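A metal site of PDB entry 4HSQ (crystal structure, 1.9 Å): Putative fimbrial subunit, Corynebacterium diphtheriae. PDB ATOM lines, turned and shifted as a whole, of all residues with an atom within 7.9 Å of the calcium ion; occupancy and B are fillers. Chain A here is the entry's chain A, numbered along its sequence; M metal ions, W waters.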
ATOM      1  N   LYS A 148     -18.309  31.597  34.384  1.00  0.00           N
ATOM      2  CA  LYS A 148     -17.627  32.616  33.573  1.00  0.00           C
ATOM      3  C   LYS A 148     -18.452  32.967  32.353  1.00  0.00           C
ATOM      4  O   LYS A 148     -19.130  32.105  31.797  1.00  0.00           O
ATOM      5  CB  LYS A 148     -16.263  32.105  33.129  1.00  0.00           C
ATOM      6  CG  LYS A 148     -15.339  31.889  34.307  1.00  0.00           C
ATOM      7  CD  LYS A 148     -13.889  31.770  33.812  1.00  0.00           C
ATOM      8  CE  LYS A 148     -13.221  30.521  34.303  1.00  0.00           C
ATOM      9  NZ  LYS A 148     -11.911  30.327  33.629  1.00  0.00           N
ATOM     10  N   ARG A 248     -27.017  27.132  35.417  1.00  0.00           N
ATOM     11  CA  ARG A 248     -26.087  26.011  35.578  1.00  0.00           C
ATOM     12  C   ARG A 248     -26.043  25.093  34.336  1.00  0.00           C
ATOM     13  O   ARG A 248     -24.962  24.745  33.854  1.00  0.00           O
ATOM     14  CB  ARG A 248     -26.478  25.173  36.810  1.00  0.00           C
ATOM     15  CG  ARG A 248     -26.211  25.869  38.154  1.00  0.00           C
ATOM     16  CD  ARG A 248     -26.741  25.057  39.309  1.00  0.00           C
ATOM     17  NE  ARG A 248     -28.191  24.887  39.263  1.00  0.00           N
ATOM     18  CZ  ARG A 248     -28.861  23.998  39.985  1.00  0.00           C
ATOM     19  NH1 ARG A 248     -28.216  23.207  40.842  1.00  0.00           N
ATOM     20  NH2 ARG A 248     -30.167  23.874  39.860  1.00  0.00           N
ATOM     21  N   ALA A 249     -27.231  24.693  33.843  1.00  0.00           N
ATOM     22  CA  ALA A 249     -27.351  23.784  32.688  1.00  0.00           C
ATOM     23  C   ALA A 249     -26.786  24.410  31.425  1.00  0.00           C
ATOM     24  O   ALA A 249     -26.035  23.730  30.693  1.00  0.00           O
ATOM     25  CB  ALA A 249     -28.802  23.376  32.479  1.00  0.00           C
ATOM     26  N   LYS A 250     -27.072  25.705  31.168  1.00  0.00           N
ATOM     27  CA  LYS A 250     -26.535  26.378  29.964  1.00  0.00           C
ATOM     28  C   LYS A 250     -25.005  26.544  30.037  1.00  0.00           C
ATOM     29  O   LYS A 250     -24.314  26.314  29.048  1.00  0.00           O
ATOM     30  CB  LYS A 250     -27.183  27.754  29.728  1.00  0.00           C
ATOM     31  CG  LYS A 250     -28.625  27.673  29.208  1.00  0.00           C
ATOM     32  CD  LYS A 250     -28.698  27.441  27.688  1.00  0.00           C
ATOM     33  CE  LYS A 250     -30.119  27.340  27.182  1.00  0.00           C
ATOM     34  NZ  LYS A 250     -30.833  28.646  27.244  1.00  0.00           N
ATOM     35  N   ILE A 251     -24.484  26.859  31.200  1.00  0.00           N
ATOM     36  CA  ILE A 251     -23.034  27.052  31.408  1.00  0.00           C
ATOM     37  C   ILE A 251     -22.302  25.723  31.222  1.00  0.00           C
ATOM     38  O   ILE A 251     -21.248  25.676  30.591  1.00  0.00           O
ATOM     39  CB  ILE A 251     -22.788  27.639  32.807  1.00  0.00           C
ATOM     40  CG1 ILE A 251     -23.367  29.057  32.927  1.00  0.00           C
ATOM     41  CG2 ILE A 251     -21.282  27.582  33.206  1.00  0.00           C
ATOM     42  CD1 ILE A 251     -23.524  29.558  34.379  1.00  0.00           C
ATOM     43  N   SER A 252     -22.889  24.646  31.768  1.00  0.00           N
ATOM     44  CA  SER A 252     -22.339  23.273  31.754  1.00  0.00           C
ATOM     45  C   SER A 252     -22.131  22.735  30.326  1.00  0.00           C
ATOM     46  O   SER A 252     -21.256  21.905  30.141  1.00  0.00           O
ATOM     47  CB  SER A 252     -23.274  22.318  32.475  1.00  0.00           C
ATOM     48  OG  SER A 252     -22.639  21.060  32.455  1.00  0.00           O
ATOM     49  N   GLU A 253     -22.948  23.184  29.350  1.00  0.00           N
ATOM     50  CA  GLU A 253     -22.762  22.735  27.939  1.00  0.00           C
ATOM     51  C   GLU A 253     -21.328  22.983  27.499  1.00  0.00           C
ATOM     52  O   GLU A 253     -20.699  23.938  27.961  1.00  0.00           O
ATOM     53  CB  GLU A 253     -23.707  23.454  26.997  1.00  0.00           C
ATOM     54  CG  GLU A 253     -25.134  22.993  27.148  1.00  0.00           C
ATOM     55  CD  GLU A 253     -26.012  23.388  25.982  1.00  0.00           C
ATOM     56  OE1 GLU A 253     -25.900  22.764  24.904  1.00  0.00           O
ATOM     57  OE2 GLU A 253     -26.817  24.332  26.152  1.00  0.00           O
ATOM     58  N   LYS A 254     -20.766  22.115  26.656  1.00  0.00           N
ATOM     59  CA  LYS A 254     -19.395  22.341  26.266  1.00  0.00           C
ATOM     60  C   LYS A 254     -19.115  21.961  24.823  1.00  0.00           C
ATOM     61  O   LYS A 254     -19.902  21.258  24.192  1.00  0.00           O
ATOM     62  CB  LYS A 254     -18.397  21.638  27.209  1.00  0.00           C
ATOM     63  CG  LYS A 254     -18.664  20.206  27.559  1.00  0.00           C
ATOM     64  CD  LYS A 254     -17.639  19.782  28.591  1.00  0.00           C
ATOM     65  CE  LYS A 254     -17.713  18.311  28.934  1.00  0.00           C
ATOM     66  NZ  LYS A 254     -17.131  17.473  27.843  1.00  0.00           N
ATOM     67  N   ASP A 255     -17.985  22.485  24.323  1.00  0.00           N
ATOM     68  CA  ASP A 255     -17.435  22.244  22.979  1.00  0.00           C
ATOM     69  C   ASP A 255     -18.359  22.709  21.841  1.00  0.00           C
ATOM     70  O   ASP A 255     -18.312  22.147  20.745  1.00  0.00           O
ATOM     71  CB  ASP A 255     -17.059  20.766  22.824  1.00  0.00           C
ATOM     72  CG  ASP A 255     -15.930  20.346  23.741  1.00  0.00           C
ATOM     73  OD1 ASP A 255     -14.912  21.087  23.824  1.00  0.00           O
ATOM     74  OD2 ASP A 255     -16.028  19.262  24.336  1.00  0.00           O
ATOM     75  N   LYS A 256     -19.149  23.763  22.097  1.00  0.00           N
ATOM     76  CA  LYS A 256     -20.050  24.358  21.097  1.00  0.00           C
ATOM     77  C   LYS A 256     -19.369  25.573  20.449  1.00  0.00           C
ATOM     78  O   LYS A 256     -19.784  25.995  19.389  1.00  0.00           O
ATOM     79  CB  LYS A 256     -21.407  24.757  21.707  1.00  0.00           C
ATOM     80  CG  LYS A 256     -22.132  23.633  22.474  1.00  0.00           C
ATOM     81  CD  LYS A 256     -22.377  22.394  21.589  1.00  0.00           C
ATOM     82  CE  LYS A 256     -23.077  21.277  22.315  1.00  0.00           C
ATOM     83  NZ  LYS A 256     -23.329  20.142  21.387  1.00  0.00           N
ATOM     84  N   PHE A 257     -18.347  26.126  21.116  1.00  0.00           N
ATOM     85  CA  PHE A 257     -17.531  27.267  20.694  1.00  0.00           C
ATOM     86  C   PHE A 257     -16.125  27.104  21.221  1.00  0.00           C
ATOM     87  O   PHE A 257     -15.952  26.416  22.215  1.00  0.00           O
ATOM     88  CB  PHE A 257     -18.090  28.588  21.275  1.00  0.00           C
ATOM     89  CG  PHE A 257     -19.538  28.875  21.090  1.00  0.00           C
ATOM     90  CD1 PHE A 257     -19.985  29.611  20.000  1.00  0.00           C
ATOM     91  CD2 PHE A 257     -20.471  28.457  22.037  1.00  0.00           C
ATOM     92  CE1 PHE A 257     -21.341  29.890  19.845  1.00  0.00           C
ATOM     93  CE2 PHE A 257     -21.821  28.752  21.879  1.00  0.00           C
ATOM     94  CZ  PHE A 257     -22.240  29.484  20.800  1.00  0.00           C
ATOM     95  N   GLY A 259     -13.210  27.620  23.615  1.00  0.00           N
ATOM     96  CA  GLY A 259     -13.197  28.046  25.015  1.00  0.00           C
ATOM     97  C   GLY A 259     -14.457  27.701  25.780  1.00  0.00           C
ATOM     98  O   GLY A 259     -14.617  28.080  26.940  1.00  0.00           O
ATOM     99  N   ASP A 260     -15.357  26.914  25.159  1.00  0.00           N
ATOM    100  CA  ASP A 260     -16.605  26.525  25.780  1.00  0.00           C
ATOM    101  C   ASP A 260     -16.414  25.328  26.704  1.00  0.00           C
ATOM    102  O   ASP A 260     -16.598  24.172  26.278  1.00  0.00           O
ATOM    103  CB  ASP A 260     -17.671  26.212  24.717  1.00  0.00           C
ATOM    104  CG  ASP A 260     -19.043  25.936  25.285  1.00  0.00           C
ATOM    105  OD1 ASP A 260     -19.278  26.287  26.461  1.00  0.00           O
ATOM    106  OD2 ASP A 260     -19.893  25.397  24.535  1.00  0.00           O
ATOM    107  N   ASP A 261     -16.038  25.576  27.937  1.00  0.00           N
ATOM    108  CA  ASP A 261     -15.884  24.487  28.876  1.00  0.00           C
ATOM    109  C   ASP A 261     -17.122  24.451  29.787  1.00  0.00           C
ATOM    110  O   ASP A 261     -18.075  25.214  29.559  1.00  0.00           O
ATOM    111  CB  ASP A 261     -14.560  24.579  29.641  1.00  0.00           C
ATOM    112  CG  ASP A 261     -14.386  25.816  30.488  1.00  0.00           C
ATOM    113  OD1 ASP A 261     -15.395  26.367  30.923  1.00  0.00           O
ATOM    114  OD2 ASP A 261     -13.229  26.166  30.809  1.00  0.00           O
ATOM    115  N   GLU A 262     -17.134  23.560  30.769  1.00  0.00           N
ATOM    116  CA  GLU A 262     -18.303  23.383  31.619  1.00  0.00           C
ATOM    117  C   GLU A 262     -18.487  24.499  32.684  1.00  0.00           C
ATOM    118  O   GLU A 262     -19.499  24.461  33.373  1.00  0.00           O
ATOM    119  CB  GLU A 262     -18.263  21.972  32.275  1.00  0.00           C
ATOM    120  CG  GLU A 262     -17.160  21.769  33.312  1.00  0.00           C
ATOM    121  CD  GLU A 262     -15.840  21.249  32.788  1.00  0.00           C
ATOM    122  OE1 GLU A 262     -15.464  21.553  31.629  1.00  0.00           O
ATOM    123  OE2 GLU A 262     -15.150  20.536  33.556  1.00  0.00           O
ATOM    124  N   VAL A 263     -17.548  25.483  32.802  1.00  0.00           N
ATOM    125  CA  VAL A 263     -17.696  26.567  33.804  1.00  0.00           C
ATOM    126  C   VAL A 263     -17.883  27.935  33.096  1.00  0.00           C
ATOM    127  O   VAL A 263     -17.958  28.978  33.766  1.00  0.00           O
ATOM    128  CB  VAL A 263     -16.520  26.627  34.850  1.00  0.00           C
ATOM    129  CG1 VAL A 263     -16.388  25.317  35.612  1.00  0.00           C
ATOM    130  CG2 VAL A 263     -15.177  27.006  34.187  1.00  0.00           C
ATOM    131  N   THR A 264     -17.920  27.925  31.762  1.00  0.00           N
ATOM    132  CA  THR A 264     -18.007  29.126  30.925  1.00  0.00           C
ATOM    133  C   THR A 264     -19.152  29.051  29.943  1.00  0.00           C
ATOM    134  O   THR A 264     -19.339  28.059  29.257  1.00  0.00           O
ATOM    135  CB  THR A 264     -16.684  29.324  30.132  1.00  0.00           C
ATOM    136  OG1 THR A 264     -15.566  29.157  31.016  1.00  0.00           O
ATOM    137  CG2 THR A 264     -16.605  30.708  29.431  1.00  0.00           C
ATOM    138  N   LEU A 265     -19.881  30.144  29.849  1.00  0.00           N
ATOM    139  CA  LEU A 265     -20.883  30.320  28.829  1.00  0.00           C
ATOM    140  C   LEU A 265     -20.236  31.228  27.809  1.00  0.00           C
ATOM    141  O   LEU A 265     -19.672  32.242  28.200  1.00  0.00           O
ATOM    142  CB  LEU A 265     -22.152  30.931  29.409  1.00  0.00           C
ATOM    143  CG  LEU A 265     -23.359  30.944  28.455  1.00  0.00           C
ATOM    144  CD1 LEU A 265     -24.634  30.647  29.235  1.00  0.00           C
ATOM    145  CD2 LEU A 265     -23.508  32.282  27.769  1.00  0.00           C
ATOM    146  N   VAL A 266     -20.296  30.849  26.530  1.00  0.00           N
ATOM    147  CA  VAL A 266     -19.705  31.630  25.449  1.00  0.00           C
ATOM    148  C   VAL A 266     -20.837  32.284  24.658  1.00  0.00           C
ATOM    149  O   VAL A 266     -21.753  31.597  24.198  1.00  0.00           O
ATOM    150  CB  VAL A 266     -18.759  30.798  24.508  1.00  0.00           C
ATOM    151  CG1 VAL A 266     -18.212  31.656  23.362  1.00  0.00           C
ATOM    152  CG2 VAL A 266     -17.618  30.155  25.272  1.00  0.00           C
HETATM  153 CA    CA M   1     -19.999  25.983  28.712  1.00  0.00          CA
HETATM  154  O   HOH W   1     -22.090  26.945  27.800  1.00  0.00           O
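The side-chain carboxylate of Asp 261 is in hydrogen-bond range of the backbone NH of Val 263.
OD2 of Asp 260 sits at hydrogen-bond distance from N of Lys 256 (3.0 Å).
The side-chain hydroxyl (OG1) of Thr 264 is in hydrogen-bond range of the side-chain carboxylate (OD1) of Asp 261, 2.8 Å away.
O of Asp 260 lies within hydrogen-bond range of N of Asp 255, 2.9 Å away.
Of the 19 residues printed, 5 come within 4 Å of the calcium ion.
The nearest printed residue that does not touch the calcium ion is Ser 252 (4.2 Å).
The calcium ion is bound by O of Asp 261 (2.2 Å), O of Thr 264 (2.2 Å), O of Ile 251 (2.3 Å), O of Glu 253 (2.3 Å), OD1 of Asp 260 (2.4 Å) and water W1 (2.5 Å).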
